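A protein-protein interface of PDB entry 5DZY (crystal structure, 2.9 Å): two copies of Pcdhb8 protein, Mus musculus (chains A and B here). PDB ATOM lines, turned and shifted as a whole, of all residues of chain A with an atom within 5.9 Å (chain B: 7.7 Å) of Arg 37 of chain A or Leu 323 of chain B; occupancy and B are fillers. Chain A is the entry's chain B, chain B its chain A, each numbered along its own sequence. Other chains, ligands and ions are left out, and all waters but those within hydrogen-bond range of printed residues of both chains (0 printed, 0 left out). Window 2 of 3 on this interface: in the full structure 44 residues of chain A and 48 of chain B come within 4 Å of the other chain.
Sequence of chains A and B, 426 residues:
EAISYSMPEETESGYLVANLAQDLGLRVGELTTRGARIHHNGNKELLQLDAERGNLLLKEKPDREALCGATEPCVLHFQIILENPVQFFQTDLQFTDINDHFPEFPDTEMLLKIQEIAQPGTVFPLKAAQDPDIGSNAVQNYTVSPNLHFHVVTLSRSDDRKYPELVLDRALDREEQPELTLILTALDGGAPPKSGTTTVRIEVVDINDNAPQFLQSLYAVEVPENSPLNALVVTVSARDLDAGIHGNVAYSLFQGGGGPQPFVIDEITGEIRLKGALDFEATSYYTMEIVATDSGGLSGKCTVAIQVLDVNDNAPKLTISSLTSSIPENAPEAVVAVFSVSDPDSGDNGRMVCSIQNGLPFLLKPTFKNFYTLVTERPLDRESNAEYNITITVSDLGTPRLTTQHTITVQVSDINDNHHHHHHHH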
ATOM      1  N   GLY A  35     -14.778  -3.456 -32.202  1.00  0.00           N
ATOM      2  CA  GLY A  35     -14.151  -2.900 -31.018  1.00  0.00           C
ATOM      3  C   GLY A  35     -15.148  -2.623 -29.911  1.00  0.00           C
ATOM      4  O   GLY A  35     -15.263  -1.494 -29.435  1.00  0.00           O
ATOM      5  N   ALA A  36     -15.877  -3.661 -29.511  1.00  0.00           N
ATOM      6  CA  ALA A  36     -16.892  -3.539 -28.472  1.00  0.00           C
ATOM      7  C   ALA A  36     -16.279  -3.092 -27.151  1.00  0.00           C
ATOM      8  O   ALA A  36     -15.364  -3.734 -26.634  1.00  0.00           O
ATOM      9  CB  ALA A  36     -17.626  -4.855 -28.295  1.00  0.00           C
ATOM     10  N   ARG A  37     -16.782  -1.987 -26.611  1.00  0.00           N
ATOM     11  CA  ARG A  37     -16.270  -1.464 -25.350  1.00  0.00           C
ATOM     12  C   ARG A  37     -17.388  -1.226 -24.343  1.00  0.00           C
ATOM     13  O   ARG A  37     -18.548  -1.037 -24.715  1.00  0.00           O
ATOM     14  CB  ARG A  37     -15.492  -0.169 -25.583  1.00  0.00           C
ATOM     15  CG  ARG A  37     -14.239  -0.342 -26.424  1.00  0.00           C
ATOM     16  CD  ARG A  37     -13.484   0.967 -26.551  1.00  0.00           C
ATOM     17  NE  ARG A  37     -13.159   1.534 -25.245  1.00  0.00           N
ATOM     18  CZ  ARG A  37     -12.479   2.662 -25.070  1.00  0.00           C
ATOM     19  NH1 ARG A  37     -12.229   3.106 -23.846  1.00  0.00           N
ATOM     20  NH2 ARG A  37     -12.049   3.345 -26.121  1.00  0.00           N
ATOM     21  N   ILE A  38     -17.024  -1.232 -23.066  1.00  0.00           N
ATOM     22  CA  ILE A  38     -17.984  -1.077 -21.982  1.00  0.00           C
ATOM     23  C   ILE A  38     -17.846   0.288 -21.307  1.00  0.00           C
ATOM     24  O   ILE A  38     -16.735   0.746 -21.033  1.00  0.00           O
ATOM     25  CB  ILE A  38     -17.821  -2.204 -20.932  1.00  0.00           C
ATOM     26  CG1 ILE A  38     -18.765  -1.988 -19.750  1.00  0.00           C
ATOM     27  CG2 ILE A  38     -16.375  -2.305 -20.462  1.00  0.00           C
ATOM     28  CD1 ILE A  38     -20.221  -2.018 -20.134  1.00  0.00           C
ATOM     29  N   HIS A  39     -18.975   0.942 -21.056  1.00  0.00           N
ATOM     30  CA  HIS A  39     -18.963   2.222 -20.357  1.00  0.00           C
ATOM     31  C   HIS A  39     -19.957   2.248 -19.202  1.00  0.00           C
ATOM     32  O   HIS A  39     -21.122   1.862 -19.349  1.00  0.00           O
ATOM     33  CB  HIS A  39     -19.261   3.371 -21.320  1.00  0.00           C
ATOM     34  CG  HIS A  39     -19.093   4.727 -20.706  1.00  0.00           C
ATOM     35  ND1 HIS A  39     -19.745   5.847 -21.177  1.00  0.00           N
ATOM     36  CD2 HIS A  39     -18.338   5.144 -19.661  1.00  0.00           C
ATOM     37  CE1 HIS A  39     -19.404   6.893 -20.446  1.00  0.00           C
ATOM     38  NE2 HIS A  39     -18.552   6.494 -19.520  1.00  0.00           N
ATOM     39  N   LEU A  49     -15.352  -6.802 -20.361  1.00  0.00           N
ATOM     40  CA  LEU A  49     -15.843  -7.379 -21.605  1.00  0.00           C
ATOM     41  C   LEU A  49     -14.825  -8.307 -22.261  1.00  0.00           C
ATOM     42  O   LEU A  49     -13.665  -7.941 -22.450  1.00  0.00           O
ATOM     43  CB  LEU A  49     -16.240  -6.269 -22.579  1.00  0.00           C
ATOM     44  CG  LEU A  49     -16.872  -6.719 -23.896  1.00  0.00           C
ATOM     45  CD1 LEU A  49     -18.030  -7.666 -23.633  1.00  0.00           C
ATOM     46  CD2 LEU A  49     -17.336  -5.513 -24.693  1.00  0.00           C
ATOM     47  N   GLN A  79     -23.656   0.918 -20.496  1.00  0.00           N
ATOM     48  CA  GLN A  79     -23.826   0.982 -21.942  1.00  0.00           C
ATOM     49  C   GLN A  79     -22.689   0.295 -22.688  1.00  0.00           C
ATOM     50  O   GLN A  79     -21.540   0.304 -22.243  1.00  0.00           O
ATOM     51  CB  GLN A  79     -23.947   2.436 -22.404  1.00  0.00           C
ATOM     52  CG  GLN A  79     -22.853   3.353 -21.884  1.00  0.00           C
ATOM     53  CD  GLN A  79     -23.154   3.900 -20.501  1.00  0.00           C
ATOM     54  OE1 GLN A  79     -24.197   3.605 -19.918  1.00  0.00           O
ATOM     55  NE2 GLN A  79     -22.238   4.701 -19.969  1.00  0.00           N
ATOM     56  N   ILE A  80     -23.022  -0.298 -23.829  1.00  0.00           N
ATOM     57  CA  ILE A  80     -22.043  -0.984 -24.661  1.00  0.00           C
ATOM     58  C   ILE A  80     -21.897  -0.265 -25.994  1.00  0.00           C
ATOM     59  O   ILE A  80     -22.884  -0.045 -26.696  1.00  0.00           O
ATOM     60  CB  ILE A  80     -22.445  -2.446 -24.915  1.00  0.00           C
ATOM     61  CG1 ILE A  80     -22.896  -3.106 -23.611  1.00  0.00           C
ATOM     62  CG2 ILE A  80     -21.296  -3.212 -25.551  1.00  0.00           C
ATOM     63  CD1 ILE A  80     -23.612  -4.418 -23.810  1.00  0.00           C
ATOM     64  N   ILE A  81     -20.669   0.102 -26.347  1.00  0.00           N
ATOM     65  CA  ILE A  81     -20.445   0.844 -27.582  1.00  0.00           C
ATOM     66  C   ILE A  81     -19.700   0.021 -28.632  1.00  0.00           C
ATOM     67  O   ILE A  81     -18.806  -0.768 -28.313  1.00  0.00           O
ATOM     68  CB  ILE A  81     -19.676   2.161 -27.316  1.00  0.00           C
ATOM     69  CG1 ILE A  81     -18.276   1.882 -26.764  1.00  0.00           C
ATOM     70  CG2 ILE A  81     -20.457   3.050 -26.360  1.00  0.00           C
ATOM     71  CD1 ILE A  81     -17.162   2.209 -27.739  1.00  0.00           C
ATOM     72  N   LEU A  82     -20.099   0.205 -29.888  1.00  0.00           N
ATOM     73  CA  LEU A  82     -19.455  -0.443 -31.023  1.00  0.00           C
ATOM     74  C   LEU A  82     -18.911   0.631 -31.959  1.00  0.00           C
ATOM     75  O   LEU A  82     -19.419   1.752 -31.973  1.00  0.00           O
ATOM     76  CB  LEU A  82     -20.439  -1.355 -31.758  1.00  0.00           C
ATOM     77  CG  LEU A  82     -21.258  -2.311 -30.886  1.00  0.00           C
ATOM     78  CD1 LEU A  82     -22.215  -3.132 -31.736  1.00  0.00           C
ATOM     79  CD2 LEU A  82     -20.349  -3.216 -30.072  1.00  0.00           C
ATOM     80  N   GLU A  83     -17.891   0.293 -32.742  1.00  0.00           N
ATOM     81  CA  GLU A  83     -17.205   1.295 -33.555  1.00  0.00           C
ATOM     82  C   GLU A  83     -17.115   0.945 -35.041  1.00  0.00           C
ATOM     83  O   GLU A  83     -16.417   1.622 -35.796  1.00  0.00           O
ATOM     84  CB  GLU A  83     -15.795   1.531 -33.006  1.00  0.00           C
ATOM     85  N   VAL A  86     -20.331   3.112 -35.568  1.00  0.00           N
ATOM     86  CA  VAL A  86     -20.614   3.550 -34.207  1.00  0.00           C
ATOM     87  C   VAL A  86     -22.034   3.173 -33.794  1.00  0.00           C
ATOM     88  O   VAL A  86     -22.995   3.445 -34.514  1.00  0.00           O
ATOM     89  CB  VAL A  86     -20.417   5.071 -34.048  1.00  0.00           C
ATOM     90  CG1 VAL A  86     -18.939   5.401 -33.900  1.00  0.00           C
ATOM     91  CG2 VAL A  86     -21.027   5.818 -35.227  1.00  0.00           C
ATOM     92  N   PHE A  88     -24.688   2.312 -30.049  1.00  0.00           N
ATOM     93  CA  PHE A  88     -24.841   2.372 -28.598  1.00  0.00           C
ATOM     94  C   PHE A  88     -25.956   1.452 -28.106  1.00  0.00           C
ATOM     95  O   PHE A  88     -27.056   1.446 -28.658  1.00  0.00           O
ATOM     96  CB  PHE A  88     -25.117   3.809 -28.153  1.00  0.00           C
ATOM     97  CG  PHE A  88     -24.214   4.826 -28.790  1.00  0.00           C
ATOM     98  CD1 PHE A  88     -22.952   5.072 -28.275  1.00  0.00           C
ATOM     99  CD2 PHE A  88     -24.628   5.537 -29.905  1.00  0.00           C
ATOM    100  CE1 PHE A  88     -22.119   6.008 -28.860  1.00  0.00           C
ATOM    101  CE2 PHE A  88     -23.800   6.474 -30.495  1.00  0.00           C
ATOM    102  CZ  PHE A  88     -22.544   6.709 -29.972  1.00  0.00           C
ATOM    103  N   ILE B 320     -15.446  10.124 -18.508  1.00  0.00           N
ATOM    104  CA  ILE B 320     -15.225  10.079 -19.949  1.00  0.00           C
ATOM    105  C   ILE B 320     -14.448   8.844 -20.400  1.00  0.00           C
ATOM    106  O   ILE B 320     -13.416   8.501 -19.826  1.00  0.00           O
ATOM    107  CB  ILE B 320     -14.466  11.333 -20.430  1.00  0.00           C
ATOM    108  CG1 ILE B 320     -15.047  12.593 -19.783  1.00  0.00           C
ATOM    109  CG2 ILE B 320     -14.498  11.432 -21.950  1.00  0.00           C
ATOM    110  CD1 ILE B 320     -14.319  13.863 -20.157  1.00  0.00           C
ATOM    111  N   SER B 321     -14.958   8.186 -21.435  1.00  0.00           N
ATOM    112  CA  SER B 321     -14.254   7.090 -22.087  1.00  0.00           C
ATOM    113  C   SER B 321     -13.982   7.451 -23.545  1.00  0.00           C
ATOM    114  O   SER B 321     -14.909   7.731 -24.311  1.00  0.00           O
ATOM    115  CB  SER B 321     -15.059   5.791 -21.993  1.00  0.00           C
ATOM    116  OG  SER B 321     -16.340   5.941 -22.578  1.00  0.00           O
ATOM    117  N   SER B 322     -12.708   7.450 -23.922  1.00  0.00           N
ATOM    118  CA  SER B 322     -12.300   7.863 -25.260  1.00  0.00           C
ATOM    119  C   SER B 322     -12.306   6.703 -26.248  1.00  0.00           C
ATOM    120  O   SER B 322     -11.869   5.599 -25.927  1.00  0.00           O
ATOM    121  CB  SER B 322     -10.910   8.500 -25.216  1.00  0.00           C
ATOM    122  OG  SER B 322     -10.481   8.876 -26.513  1.00  0.00           O
ATOM    123  N   LEU B 323     -12.801   6.964 -27.455  1.00  0.00           N
ATOM    124  CA  LEU B 323     -12.840   5.952 -28.505  1.00  0.00           C
ATOM    125  C   LEU B 323     -11.586   6.008 -29.369  1.00  0.00           C
ATOM    126  O   LEU B 323     -10.928   4.992 -29.595  1.00  0.00           O
ATOM    127  CB  LEU B 323     -14.082   6.126 -29.387  1.00  0.00           C
ATOM    128  CG  LEU B 323     -15.444   5.677 -28.848  1.00  0.00           C
ATOM    129  CD1 LEU B 323     -15.964   6.634 -27.791  1.00  0.00           C
ATOM    130  CD2 LEU B 323     -16.444   5.539 -29.986  1.00  0.00           C
ATOM    131  N   THR B 324     -11.264   7.203 -29.853  1.00  0.00           N
ATOM    132  CA  THR B 324     -10.125   7.390 -30.743  1.00  0.00           C
ATOM    133  C   THR B 324      -9.113   8.374 -30.168  1.00  0.00           C
ATOM    134  O   THR B 324      -9.416   9.552 -29.982  1.00  0.00           O
ATOM    135  CB  THR B 324     -10.576   7.891 -32.127  1.00  0.00           C
ATOM    136  OG1 THR B 324     -11.302   9.118 -31.978  1.00  0.00           O
ATOM    137  CG2 THR B 324     -11.466   6.860 -32.805  1.00  0.00           C
ATOM    138  N   SER B 325      -7.910   7.882 -29.887  1.00  0.00           N
ATOM    139  CA  SER B 325      -6.829   8.731 -29.403  1.00  0.00           C
ATOM    140  C   SER B 325      -6.411   9.719 -30.486  1.00  0.00           C
ATOM    141  O   SER B 325      -6.216  10.906 -30.221  1.00  0.00           O
ATOM    142  CB  SER B 325      -5.632   7.885 -28.965  1.00  0.00           C
ATOM    143  OG  SER B 325      -5.127   7.118 -30.044  1.00  0.00           O
ATOM    144  N   SER B 326      -6.279   9.217 -31.709  1.00  0.00           N
ATOM    145  CA  SER B 326      -5.981  10.055 -32.863  1.00  0.00           C
ATOM    146  C   SER B 326      -7.116   9.967 -33.876  1.00  0.00           C
ATOM    147  O   SER B 326      -7.918   9.035 -33.840  1.00  0.00           O
ATOM    148  CB  SER B 326      -4.657   9.640 -33.506  1.00  0.00           C
ATOM    149  OG  SER B 326      -3.582   9.781 -32.593  1.00  0.00           O
ATOM    150  N   ALA B 334     -16.616  12.026 -37.019  1.00  0.00           N
ATOM    151  CA  ALA B 334     -15.908  11.005 -36.256  1.00  0.00           C
ATOM    152  C   ALA B 334     -16.125  11.187 -34.758  1.00  0.00           C
ATOM    153  O   ALA B 334     -16.022  12.298 -34.236  1.00  0.00           O
ATOM    154  CB  ALA B 334     -14.424  11.033 -36.585  1.00  0.00           C
ATOM    155  N   VAL B 335     -16.426  10.090 -34.072  1.00  0.00           N
ATOM    156  CA  VAL B 335     -16.659  10.124 -32.635  1.00  0.00           C
ATOM    157  C   VAL B 335     -15.345  10.090 -31.862  1.00  0.00           C
ATOM    158  O   VAL B 335     -14.660   9.067 -31.830  1.00  0.00           O
ATOM    159  CB  VAL B 335     -17.545   8.949 -32.180  1.00  0.00           C
ATOM    160  CG1 VAL B 335     -17.755   8.996 -30.674  1.00  0.00           C
ATOM    161  CG2 VAL B 335     -18.878   8.976 -32.911  1.00  0.00           C
ATOM    162  N   VAL B 336     -14.999  11.212 -31.244  1.00  0.00           N
ATOM    163  CA  VAL B 336     -13.765  11.316 -30.473  1.00  0.00           C
ATOM    164  C   VAL B 336     -13.860  10.538 -29.166  1.00  0.00           C
ATOM    165  O   VAL B 336     -13.074   9.624 -28.915  1.00  0.00           O
ATOM    166  CB  VAL B 336     -13.417  12.782 -30.159  1.00  0.00           C
ATOM    167  CG1 VAL B 336     -12.176  12.857 -29.283  1.00  0.00           C
ATOM    168  CG2 VAL B 336     -13.219  13.567 -31.445  1.00  0.00           C
ATOM    169  N   ALA B 337     -14.828  10.907 -28.334  1.00  0.00           N
ATOM    170  CA  ALA B 337     -15.009  10.262 -27.040  1.00  0.00           C
ATOM    171  C   ALA B 337     -16.469  10.293 -26.606  1.00  0.00           C
ATOM    172  O   ALA B 337     -17.232  11.167 -27.021  1.00  0.00           O
ATOM    173  CB  ALA B 337     -14.135  10.930 -25.991  1.00  0.00           C
ATOM    174  N   VAL B 338     -16.854   9.332 -25.774  1.00  0.00           N
ATOM    175  CA  VAL B 338     -18.196   9.316 -25.210  1.00  0.00           C
ATOM    176  C   VAL B 338     -18.106   9.461 -23.692  1.00  0.00           C
ATOM    177  O   VAL B 338     -17.235   8.871 -23.057  1.00  0.00           O
ATOM    178  CB  VAL B 338     -18.965   8.024 -25.589  1.00  0.00           C
ATOM    179  CG1 VAL B 338     -18.267   6.785 -25.044  1.00  0.00           C
ATOM    180  CG2 VAL B 338     -20.392   8.093 -25.093  1.00  0.00           C
ATOM    181  N   PHE B 339     -18.988  10.268 -23.113  1.00  0.00           N
ATOM    182  CA  PHE B 339     -18.941  10.509 -21.675  1.00  0.00           C
ATOM    183  C   PHE B 339     -20.325  10.523 -21.039  1.00  0.00           C
ATOM    184  O   PHE B 339     -21.332  10.749 -21.710  1.00  0.00           O
ATOM    185  CB  PHE B 339     -18.219  11.827 -21.378  1.00  0.00           C
ATOM    186  CG  PHE B 339     -18.903  13.042 -21.940  1.00  0.00           C
ATOM    187  CD1 PHE B 339     -19.824  13.748 -21.183  1.00  0.00           C
ATOM    188  CD2 PHE B 339     -18.617  13.486 -23.220  1.00  0.00           C
ATOM    189  CE1 PHE B 339     -20.452  14.868 -21.695  1.00  0.00           C
ATOM    190  CE2 PHE B 339     -19.241  14.605 -23.736  1.00  0.00           C
ATOM    191  CZ  PHE B 339     -20.159  15.297 -22.972  1.00  0.00           C
ATOM    192  N   THR B 373     -22.283  12.256 -26.428  1.00  0.00           N
ATOM    193  CA  THR B 373     -21.182  11.831 -27.289  1.00  0.00           C
ATOM    194  C   THR B 373     -20.493  13.032 -27.931  1.00  0.00           C
ATOM    195  O   THR B 373     -21.154  13.944 -28.428  1.00  0.00           O
ATOM    196  CB  THR B 373     -21.658  10.878 -28.405  1.00  0.00           C
ATOM    197  OG1 THR B 373     -22.641  11.537 -29.214  1.00  0.00           O
ATOM    198  CG2 THR B 373     -22.258   9.614 -27.812  1.00  0.00           C
ATOM    199  N   LEU B 374     -19.165  13.027 -27.917  1.00  0.00           N
ATOM    200  CA  LEU B 374     -18.392  14.109 -28.516  1.00  0.00           C
ATOM    201  C   LEU B 374     -17.947  13.739 -29.927  1.00  0.00           C
ATOM    202  O   LEU B 374     -17.042  12.925 -30.109  1.00  0.00           O
ATOM    203  CB  LEU B 374     -17.181  14.449 -27.645  1.00  0.00           C
ATOM    204  CG  LEU B 374     -16.274  15.572 -28.152  1.00  0.00           C
ATOM    205  CD1 LEU B 374     -17.076  16.836 -28.412  1.00  0.00           C
ATOM    206  CD2 LEU B 374     -15.154  15.844 -27.163  1.00  0.00           C
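The backbone carbonyl oxygen (O) of Ser 322 of chain B sits close to the guanidinium group (NH1) of Arg 37 of chain A (3.3 Å).
The backbone NH (N) of Ser 321 of chain B is in hydrogen-bond range of the backbone carbonyl oxygen (O) of Val 338 of chain B (2.9 Å).
N of Leu 323 of chain B sits at hydrogen-bond distance from O of Val 336 of chain B, at 3.0 Å.
N of Ile 81 of chain A is in hydrogen-bond range of O of Arg 37 of chain A (2.9 Å).
O of Gln 79 of chain A sits at hydrogen-bond distance from N of His 39 of chain A (2.9 Å).
The side-chain hydroxyl of Thr 324 of chain B is in hydrogen-bond range of the backbone carbonyl oxygen of Val 335 of chain B, 3.4 Å away.
NH2 of Arg 37 of chain A touches CA of Leu 323 of chain B, at 3.6 Å.
Ser 321 of chain B touches His 39 of chain A.
Val 338 of chain B touches His 39 of chain A (O to CE1, 3.9 Å).
His 39 of chain A touches Phe 339 of chain B.
Val 86 of chain A touches Val 335 of chain B (CG1 to CG2, 3.7 Å).
Phe 88 of chain A touches Thr 373 of chain B (CZ to CG2, 3.6 Å).
No residue of chain B comes within 4 Å of Ala 36 of chain A.
Arg 37 of chain A touches two residues of chain B.
Of the printed residues of chain B, Phe 88 of chain A touches Thr 373 (3.6 Å).
Of chain A, only Arg 37 comes within 4 Å of Leu 323 of chain B.
Of the printed residues of chain A, Val 338 of chain B touches His 39 (3.9 Å).
Of the printed residues of chain A, Phe 339 of chain B touches His 39 (3.8 Å).
Of the printed residues of chain A, Thr 373 of chain B touches Phe 88 (3.6 Å).
Hydrophobic or aromatic side chains of chain A that line the printed part of chain B: His 39, Val 86 and Phe 88.
Of the 15 printed residues of chain B, 7 touch a printed residue of chain A.
Hydrophobic or aromatic side chains of chain B that line the printed part of chain A: Val 335.
Among the printed residues, no Asp or Glu carboxylate lies within 4 Å of a Lys or Arg side-chain nitrogen of the other chain.
No position is printed for both chains.
Of the 7 pairs that touch across the chains among the printed residues, none has its exchanged pair printed and touching as well.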
